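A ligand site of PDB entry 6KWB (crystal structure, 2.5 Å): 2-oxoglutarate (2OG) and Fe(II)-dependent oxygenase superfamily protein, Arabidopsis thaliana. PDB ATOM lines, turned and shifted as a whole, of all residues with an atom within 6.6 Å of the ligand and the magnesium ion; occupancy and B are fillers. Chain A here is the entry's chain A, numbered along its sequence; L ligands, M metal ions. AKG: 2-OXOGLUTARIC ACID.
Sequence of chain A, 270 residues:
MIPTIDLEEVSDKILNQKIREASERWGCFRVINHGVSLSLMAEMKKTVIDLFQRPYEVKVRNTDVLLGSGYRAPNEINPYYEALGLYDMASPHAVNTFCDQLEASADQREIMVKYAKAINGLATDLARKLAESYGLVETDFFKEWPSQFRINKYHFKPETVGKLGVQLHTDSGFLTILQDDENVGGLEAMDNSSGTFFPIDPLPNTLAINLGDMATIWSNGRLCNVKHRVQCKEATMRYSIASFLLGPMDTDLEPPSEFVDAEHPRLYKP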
ATOM      1  N   TYR A  81      18.281 -23.398  -4.936  1.00  0.00           N
ATOM      2  CA  TYR A  81      17.278 -24.293  -4.388  1.00  0.00           C
ATOM      3  C   TYR A  81      17.119 -25.532  -5.252  1.00  0.00           C
ATOM      4  O   TYR A  81      16.992 -25.443  -6.462  1.00  0.00           O
ATOM      5  CB  TYR A  81      15.953 -23.529  -4.232  1.00  0.00           C
ATOM      6  CG  TYR A  81      14.740 -24.345  -3.796  1.00  0.00           C
ATOM      7  CD1 TYR A  81      14.626 -24.827  -2.489  1.00  0.00           C
ATOM      8  CD2 TYR A  81      13.685 -24.609  -4.674  1.00  0.00           C
ATOM      9  CE1 TYR A  81      13.508 -25.576  -2.076  1.00  0.00           C
ATOM     10  CE2 TYR A  81      12.579 -25.348  -4.279  1.00  0.00           C
ATOM     11  CZ  TYR A  81      12.495 -25.832  -2.980  1.00  0.00           C
ATOM     12  OH  TYR A  81      11.388 -26.561  -2.576  1.00  0.00           O
ATOM     13  N   ARG A 150       8.143 -33.049   0.841  1.00  0.00           N
ATOM     14  CA  ARG A 150       9.086 -32.325   0.025  1.00  0.00           C
ATOM     15  C   ARG A 150      10.378 -32.087   0.797  1.00  0.00           C
ATOM     16  O   ARG A 150      10.368 -31.498   1.880  1.00  0.00           O
ATOM     17  CB  ARG A 150       8.466 -31.002  -0.464  1.00  0.00           C
ATOM     18  CG  ARG A 150       9.483 -30.017  -1.030  1.00  0.00           C
ATOM     19  CD  ARG A 150       8.992 -29.194  -2.252  1.00  0.00           C
ATOM     20  NE  ARG A 150       8.970 -30.030  -3.441  1.00  0.00           N
ATOM     21  CZ  ARG A 150       9.385 -29.650  -4.649  1.00  0.00           C
ATOM     22  NH1 ARG A 150       9.865 -28.442  -4.866  1.00  0.00           N
ATOM     23  NH2 ARG A 150       9.309 -30.518  -5.662  1.00  0.00           N
ATOM     24  N   ASN A 152      14.313 -30.544   0.687  1.00  0.00           N
ATOM     25  CA  ASN A 152      14.921 -29.412   0.016  1.00  0.00           C
ATOM     26  C   ASN A 152      16.414 -29.290   0.268  1.00  0.00           C
ATOM     27  O   ASN A 152      16.843 -29.488   1.396  1.00  0.00           O
ATOM     28  CB  ASN A 152      14.247 -28.126   0.474  1.00  0.00           C
ATOM     29  CG  ASN A 152      12.739 -28.241   0.462  1.00  0.00           C
ATOM     30  OD1 ASN A 152      12.097 -28.227  -0.593  1.00  0.00           O
ATOM     31  ND2 ASN A 152      12.154 -28.355   1.663  1.00  0.00           N
ATOM     32  N   TYR A 154      19.414 -26.427  -0.122  1.00  0.00           N
ATOM     33  CA  TYR A 154      19.806 -25.054  -0.423  1.00  0.00           C
ATOM     34  C   TYR A 154      21.308 -24.894  -0.600  1.00  0.00           C
ATOM     35  O   TYR A 154      22.089 -25.260   0.268  1.00  0.00           O
ATOM     36  CB  TYR A 154      19.344 -24.139   0.695  1.00  0.00           C
ATOM     37  CG  TYR A 154      17.871 -24.139   0.837  1.00  0.00           C
ATOM     38  CD1 TYR A 154      17.069 -23.285   0.097  1.00  0.00           C
ATOM     39  CD2 TYR A 154      17.250 -25.064   1.671  1.00  0.00           C
ATOM     40  CE1 TYR A 154      15.685 -23.318   0.224  1.00  0.00           C
ATOM     41  CE2 TYR A 154      15.886 -25.108   1.800  1.00  0.00           C
ATOM     42  CZ  TYR A 154      15.103 -24.235   1.081  1.00  0.00           C
ATOM     43  OH  TYR A 154      13.746 -24.310   1.240  1.00  0.00           O
ATOM     44  N   VAL A 166      15.263 -17.854  -0.479  1.00  0.00           N
ATOM     45  CA  VAL A 166      13.911 -17.955  -1.023  1.00  0.00           C
ATOM     46  C   VAL A 166      13.141 -16.674  -0.641  1.00  0.00           C
ATOM     47  O   VAL A 166      13.351 -16.113   0.446  1.00  0.00           O
ATOM     48  CB  VAL A 166      13.168 -19.210  -0.493  1.00  0.00           C
ATOM     49  CG1 VAL A 166      11.664 -19.121  -0.762  1.00  0.00           C
ATOM     50  CG2 VAL A 166      13.752 -20.480  -1.098  1.00  0.00           C
ATOM     51  N   HIS A 169       6.758 -15.632   1.226  1.00  0.00           N
ATOM     52  CA  HIS A 169       5.631 -16.392   0.706  1.00  0.00           C
ATOM     53  C   HIS A 169       4.790 -17.105   1.800  1.00  0.00           C
ATOM     54  O   HIS A 169       5.181 -17.162   2.978  1.00  0.00           O
ATOM     55  CB  HIS A 169       6.130 -17.421  -0.281  1.00  0.00           C
ATOM     56  CG  HIS A 169       6.858 -18.551   0.360  1.00  0.00           C
ATOM     57  ND1 HIS A 169       8.031 -18.367   1.063  1.00  0.00           N
ATOM     58  CD2 HIS A 169       6.573 -19.873   0.437  1.00  0.00           C
ATOM     59  CE1 HIS A 169       8.439 -19.532   1.531  1.00  0.00           C
ATOM     60  NE2 HIS A 169       7.586 -20.465   1.156  1.00  0.00           N
ATOM     61  N   THR A 170       3.634 -17.635   1.393  1.00  0.00           N
ATOM     62  CA  THR A 170       2.804 -18.424   2.286  1.00  0.00           C
ATOM     63  C   THR A 170       2.637 -19.829   1.749  1.00  0.00           C
ATOM     64  O   THR A 170       2.478 -20.019   0.552  1.00  0.00           O
ATOM     65  CB  THR A 170       1.410 -17.847   2.443  1.00  0.00           C
ATOM     66  OG1 THR A 170       0.704 -18.007   1.210  1.00  0.00           O
ATOM     67  CG2 THR A 170       1.445 -16.376   2.893  1.00  0.00           C
ATOM     68  N   ASP A 171       2.602 -20.826   2.621  1.00  0.00           N
ATOM     69  CA  ASP A 171       2.304 -22.176   2.126  1.00  0.00           C
ATOM     70  C   ASP A 171       0.837 -22.245   1.666  1.00  0.00           C
ATOM     71  O   ASP A 171      -0.034 -21.554   2.191  1.00  0.00           O
ATOM     72  CB  ASP A 171       2.615 -23.210   3.211  1.00  0.00           C
ATOM     73  CG  ASP A 171       4.092 -23.211   3.621  1.00  0.00           C
ATOM     74  OD1 ASP A 171       4.944 -22.755   2.824  1.00  0.00           O
ATOM     75  OD2 ASP A 171       4.392 -23.704   4.715  1.00  0.00           O
ATOM     76  N   THR A 176       1.844 -27.068   7.833  1.00  0.00           N
ATOM     77  CA  THR A 176       3.156 -27.558   7.441  1.00  0.00           C
ATOM     78  C   THR A 176       3.994 -27.933   8.663  1.00  0.00           C
ATOM     79  O   THR A 176       4.069 -27.174   9.624  1.00  0.00           O
ATOM     80  CB  THR A 176       3.960 -26.519   6.631  1.00  0.00           C
ATOM     81  OG1 THR A 176       3.229 -26.150   5.466  1.00  0.00           O
ATOM     82  CG2 THR A 176       5.350 -27.091   6.223  1.00  0.00           C
ATOM     83  N   LEU A 178       7.877 -28.700   9.561  1.00  0.00           N
ATOM     84  CA  LEU A 178       9.169 -28.474   8.960  1.00  0.00           C
ATOM     85  C   LEU A 178      10.243 -29.021   9.844  1.00  0.00           C
ATOM     86  O   LEU A 178      10.318 -28.707  11.017  1.00  0.00           O
ATOM     87  CB  LEU A 178       9.401 -26.986   8.711  1.00  0.00           C
ATOM     88  CG  LEU A 178      10.782 -26.615   8.208  1.00  0.00           C
ATOM     89  CD1 LEU A 178      10.922 -27.051   6.756  1.00  0.00           C
ATOM     90  CD2 LEU A 178      11.008 -25.125   8.360  1.00  0.00           C
ATOM     91  N   GLN A 179      11.091 -29.870   9.284  1.00  0.00           N
ATOM     92  CA  GLN A 179      12.283 -30.268   9.998  1.00  0.00           C
ATOM     93  C   GLN A 179      13.446 -29.417   9.420  1.00  0.00           C
ATOM     94  O   GLN A 179      13.959 -29.674   8.347  1.00  0.00           O
ATOM     95  CB  GLN A 179      12.503 -31.795   9.906  1.00  0.00           C
ATOM     96  CG  GLN A 179      13.733 -32.283  10.591  1.00  0.00           C
ATOM     97  CD  GLN A 179      13.943 -33.790  10.518  1.00  0.00           C
ATOM     98  OE1 GLN A 179      13.029 -34.573  10.253  1.00  0.00           O
ATOM     99  NE2 GLN A 179      15.183 -34.198  10.644  1.00  0.00           N
ATOM    100  N   ASP A 180      13.800 -28.353  10.124  1.00  0.00           N
ATOM    101  CA  ASP A 180      14.773 -27.396   9.594  1.00  0.00           C
ATOM    102  C   ASP A 180      16.152 -27.977   9.646  1.00  0.00           C
ATOM    103  O   ASP A 180      16.339 -29.151   9.958  1.00  0.00           O
ATOM    104  CB  ASP A 180      14.760 -26.080  10.378  1.00  0.00           C
ATOM    105  CG  ASP A 180      15.095 -24.864   9.490  1.00  0.00           C
ATOM    106  OD1 ASP A 180      15.554 -25.057   8.344  1.00  0.00           O
ATOM    107  OD2 ASP A 180      14.984 -23.719   9.984  1.00  0.00           O
ATOM    108  N   ASP A 181      17.146 -27.146   9.346  1.00  0.00           N
ATOM    109  CA  ASP A 181      18.506 -27.614   9.289  1.00  0.00           C
ATOM    110  C   ASP A 181      19.162 -27.294  10.611  1.00  0.00           C
ATOM    111  O   ASP A 181      19.238 -26.143  11.017  1.00  0.00           O
ATOM    112  CB  ASP A 181      19.250 -26.927   8.138  1.00  0.00           C
ATOM    113  CG  ASP A 181      20.504 -27.674   7.707  1.00  0.00           C
ATOM    114  OD1 ASP A 181      20.779 -28.775   8.237  1.00  0.00           O
ATOM    115  OD2 ASP A 181      21.223 -27.132   6.843  1.00  0.00           O
ATOM    116  N   GLY A 186      18.337 -19.425   9.472  1.00  0.00           N
ATOM    117  CA  GLY A 186      17.929 -18.498   8.428  1.00  0.00           C
ATOM    118  C   GLY A 186      16.441 -18.299   8.132  1.00  0.00           C
ATOM    119  O   GLY A 186      16.069 -17.312   7.493  1.00  0.00           O
ATOM    120  N   LEU A 187      15.585 -19.218   8.590  1.00  0.00           N
ATOM    121  CA  LEU A 187      14.151 -19.092   8.346  1.00  0.00           C
ATOM    122  C   LEU A 187      13.567 -17.865   9.070  1.00  0.00           C
ATOM    123  O   LEU A 187      13.785 -17.686  10.271  1.00  0.00           O
ATOM    124  CB  LEU A 187      13.433 -20.366   8.786  1.00  0.00           C
ATOM    125  CG  LEU A 187      11.904 -20.439   8.663  1.00  0.00           C
ATOM    126  CD1 LEU A 187      11.446 -20.494   7.218  1.00  0.00           C
ATOM    127  CD2 LEU A 187      11.398 -21.647   9.410  1.00  0.00           C
ATOM    128  N   ASN A 210       3.799 -24.443  10.676  1.00  0.00           N
ATOM    129  CA  ASN A 210       3.140 -23.200  10.273  1.00  0.00           C
ATOM    130  C   ASN A 210       1.876 -23.490   9.512  1.00  0.00           C
ATOM    131  O   ASN A 210       1.671 -24.593   8.958  1.00  0.00           O
ATOM    132  CB  ASN A 210       4.040 -22.256   9.488  1.00  0.00           C
ATOM    133  CG  ASN A 210       4.626 -22.894   8.303  1.00  0.00           C
ATOM    134  OD1 ASN A 210       3.923 -23.240   7.358  1.00  0.00           O
ATOM    135  ND2 ASN A 210       5.931 -23.071   8.337  1.00  0.00           N
ATOM    136  N   HIS A 228       6.682 -16.191   5.251  1.00  0.00           N
ATOM    137  CA  HIS A 228       8.004 -16.527   5.684  1.00  0.00           C
ATOM    138  C   HIS A 228       8.994 -16.539   4.517  1.00  0.00           C
ATOM    139  O   HIS A 228       8.630 -16.562   3.340  1.00  0.00           O
ATOM    140  CB  HIS A 228       7.996 -17.872   6.412  1.00  0.00           C
ATOM    141  CG  HIS A 228       7.364 -18.995   5.638  1.00  0.00           C
ATOM    142  ND1 HIS A 228       5.994 -19.123   5.504  1.00  0.00           N
ATOM    143  CD2 HIS A 228       7.911 -20.032   4.975  1.00  0.00           C
ATOM    144  CE1 HIS A 228       5.731 -20.201   4.786  1.00  0.00           C
ATOM    145  NE2 HIS A 228       6.865 -20.775   4.451  1.00  0.00           N
ATOM    146  N   VAL A 230      13.447 -17.815   3.800  1.00  0.00           N
ATOM    147  CA  VAL A 230      14.730 -18.242   4.330  1.00  0.00           C
ATOM    148  C   VAL A 230      15.803 -17.308   3.786  1.00  0.00           C
ATOM    149  O   VAL A 230      15.931 -17.089   2.586  1.00  0.00           O
ATOM    150  CB  VAL A 230      15.029 -19.707   3.983  1.00  0.00           C
ATOM    151  CG1 VAL A 230      14.590 -20.013   2.565  1.00  0.00           C
ATOM    152  CG2 VAL A 230      16.509 -20.004   4.177  1.00  0.00           C
ATOM    153  N   ARG A 238      22.558 -26.590   2.892  1.00  0.00           N
ATOM    154  CA  ARG A 238      21.463 -26.560   3.841  1.00  0.00           C
ATOM    155  C   ARG A 238      20.322 -27.501   3.428  1.00  0.00           C
ATOM    156  O   ARG A 238      19.896 -27.533   2.276  1.00  0.00           O
ATOM    157  CB  ARG A 238      20.965 -25.124   3.984  1.00  0.00           C
ATOM    158  CG  ARG A 238      19.998 -24.861   5.107  1.00  0.00           C
ATOM    159  CD  ARG A 238      19.574 -23.394   5.064  1.00  0.00           C
ATOM    160  NE  ARG A 238      18.894 -23.034   6.298  1.00  0.00           N
ATOM    161  CZ  ARG A 238      17.584 -23.111   6.500  1.00  0.00           C
ATOM    162  NH1 ARG A 238      16.769 -23.533   5.546  1.00  0.00           N
ATOM    163  NH2 ARG A 238      17.077 -22.767   7.685  1.00  0.00           N
ATOM    164  N   TYR A 239      19.839 -28.284   4.384  1.00  0.00           N
ATOM    165  CA  TYR A 239      18.838 -29.283   4.089  1.00  0.00           C
ATOM    166  C   TYR A 239      17.605 -29.056   4.973  1.00  0.00           C
ATOM    167  O   TYR A 239      17.725 -28.643   6.111  1.00  0.00           O
ATOM    168  CB  TYR A 239      19.424 -30.670   4.314  1.00  0.00           C
ATOM    169  CG  TYR A 239      20.519 -31.010   3.339  1.00  0.00           C
ATOM    170  CD1 TYR A 239      20.223 -31.514   2.077  1.00  0.00           C
ATOM    171  CD2 TYR A 239      21.868 -30.814   3.673  1.00  0.00           C
ATOM    172  CE1 TYR A 239      21.223 -31.822   1.186  1.00  0.00           C
ATOM    173  CE2 TYR A 239      22.879 -31.113   2.783  1.00  0.00           C
ATOM    174  CZ  TYR A 239      22.552 -31.617   1.530  1.00  0.00           C
ATOM    175  OH  TYR A 239      23.553 -31.925   0.619  1.00  0.00           O
ATOM    176  N   SER A 240      16.409 -29.253   4.448  1.00  0.00           N
ATOM    177  CA  SER A 240      15.205 -29.147   5.272  1.00  0.00           C
ATOM    178  C   SER A 240      14.169 -30.130   4.764  1.00  0.00           C
ATOM    179  O   SER A 240      14.155 -30.476   3.574  1.00  0.00           O
ATOM    180  CB  SER A 240      14.645 -27.746   5.279  1.00  0.00           C
ATOM    181  OG  SER A 240      13.823 -27.593   4.144  1.00  0.00           O
ATOM    182  N   ILE A 241      13.369 -30.640   5.664  1.00  0.00           N
ATOM    183  CA  ILE A 241      12.336 -31.576   5.288  1.00  0.00           C
ATOM    184  C   ILE A 241      10.979 -31.024   5.638  1.00  0.00           C
ATOM    185  O   ILE A 241      10.765 -30.670   6.792  1.00  0.00           O
ATOM    186  CB  ILE A 241      12.529 -32.939   5.998  1.00  0.00           C
ATOM    187  CG1 ILE A 241      13.964 -33.438   5.855  1.00  0.00           C
ATOM    188  CG2 ILE A 241      11.522 -33.924   5.503  1.00  0.00           C
ATOM    189  CD1 ILE A 241      14.434 -34.359   7.023  1.00  0.00           C
ATOM    190  N   ALA A 242      10.061 -30.992   4.685  1.00  0.00           N
ATOM    191  CA  ALA A 242       8.723 -30.419   4.916  1.00  0.00           C
ATOM    192  C   ALA A 242       7.608 -31.382   4.544  1.00  0.00           C
ATOM    193  O   ALA A 242       7.636 -31.993   3.482  1.00  0.00           O
ATOM    194  CB  ALA A 242       8.561 -29.136   4.146  1.00  0.00           C
ATOM    195  N   PHE A 244       3.486 -31.336   4.129  1.00  0.00           N
ATOM    196  CA  PHE A 244       2.364 -30.433   4.009  1.00  0.00           C
ATOM    197  C   PHE A 244       1.044 -31.189   4.128  1.00  0.00           C
ATOM    198  O   PHE A 244       0.791 -32.105   3.343  1.00  0.00           O
ATOM    199  CB  PHE A 244       2.381 -29.696   2.650  1.00  0.00           C
ATOM    200  CG  PHE A 244       3.672 -28.965   2.338  1.00  0.00           C
ATOM    201  CD1 PHE A 244       3.934 -27.714   2.879  1.00  0.00           C
ATOM    202  CD2 PHE A 244       4.577 -29.480   1.418  1.00  0.00           C
ATOM    203  CE1 PHE A 244       5.083 -27.019   2.577  1.00  0.00           C
ATOM    204  CE2 PHE A 244       5.746 -28.785   1.107  1.00  0.00           C
ATOM    205  CZ  PHE A 244       6.004 -27.555   1.697  1.00  0.00           C
HETATM  206  C1  AKG L   1       9.054 -25.225   2.373  1.00  0.00           C
HETATM  207  O1  AKG L   1       9.516 -26.304   1.914  1.00  0.00           O
HETATM  208  O2  AKG L   1       7.896 -24.817   2.063  1.00  0.00           O
HETATM  209  C2  AKG L   1       9.906 -24.384   3.307  1.00  0.00           C
HETATM  210  O5  AKG L   1       9.495 -23.264   3.620  1.00  0.00           O
HETATM  211  C3  AKG L   1      11.226 -24.961   3.796  1.00  0.00           C
HETATM  212  C4  AKG L   1      11.899 -24.106   4.859  1.00  0.00           C
HETATM  213  C5  AKG L   1      13.401 -24.381   4.894  1.00  0.00           C
HETATM  214  O3  AKG L   1      14.133 -24.006   5.862  1.00  0.00           O
HETATM  215  O4  AKG L   1      13.915 -24.990   3.916  1.00  0.00           O
HETATM  216 MG    MG M   1       7.157 -22.838   2.980  1.00  0.00          MG
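The side-chain hydroxyl (OG) of Ser 240 is in hydrogen-bond range of an oxygen (O4) of the ligand. An oxygen (O3) of the ligand lies within salt-bridge range of the guanidinium group of Arg 238 (2.7 Å). OH of Tyr 154 is in hydrogen-bond range of O4 of the ligand (2.8 Å). The side-chain carboxylate of Asp 180 sits close to an oxygen (O3) of the ligand, at 3.0 Å. The side-chain amide nitrogen (ND2) of Asn 152 sits at hydrogen-bond distance from an oxygen (O1) of the ligand, at 3.4 Å.
The side-chain carboxylate (OD2) of Asp 171 is in hydrogen-bond range of the side-chain hydroxyl (OG1) of Thr 176 (2.8 Å). OD2 of Asp 171 lies close to OD1 of Asn 210 (2.7 Å). The backbone NH of His 228 sits at hydrogen-bond distance from the backbone carbonyl oxygen of His 169, at 2.9 Å. The backbone NH (N) of Asn 152 lies within hydrogen-bond range of the backbone carbonyl oxygen (O) of Ser 240 (2.9 Å). O of Arg 238 lies within hydrogen-bond range of N of Tyr 154. The guanidinium group (NH2) of Arg 238 lies within salt-bridge range of the side-chain carboxylate (OD1) of Asp 180 (2.8 Å). OH of Tyr 81 lies within hydrogen-bond range of OD1 of Asn 152 (2.7 Å). The backbone NH of Ala 242 sits at hydrogen-bond distance from the backbone carbonyl oxygen of Arg 150, 2.9 Å away.
Residues that only touch the ligand: Leu 178 (3.6 Å), Ala 242 (3.7 Å) and Phe 244 (3.3 Å). Of the 24 residues printed, 10 come within 4 Å of the ligand.
Merely in contact with the magnesium ion: His 169 (3.0 Å). Three residues have an atom within 4 Å of the magnesium ion: His 169, Asp 171 and His 228. The nearest printed residue that does not touch the magnesium ion is Phe 244 (4.7 Å).
The magnesium ion is bound by OD1 of Asp 171 (2.2 Å), O2 of the ligand (2.3 Å), O5 of the ligand (2.5 Å) and NE2 of His 228 (2.6 Å).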
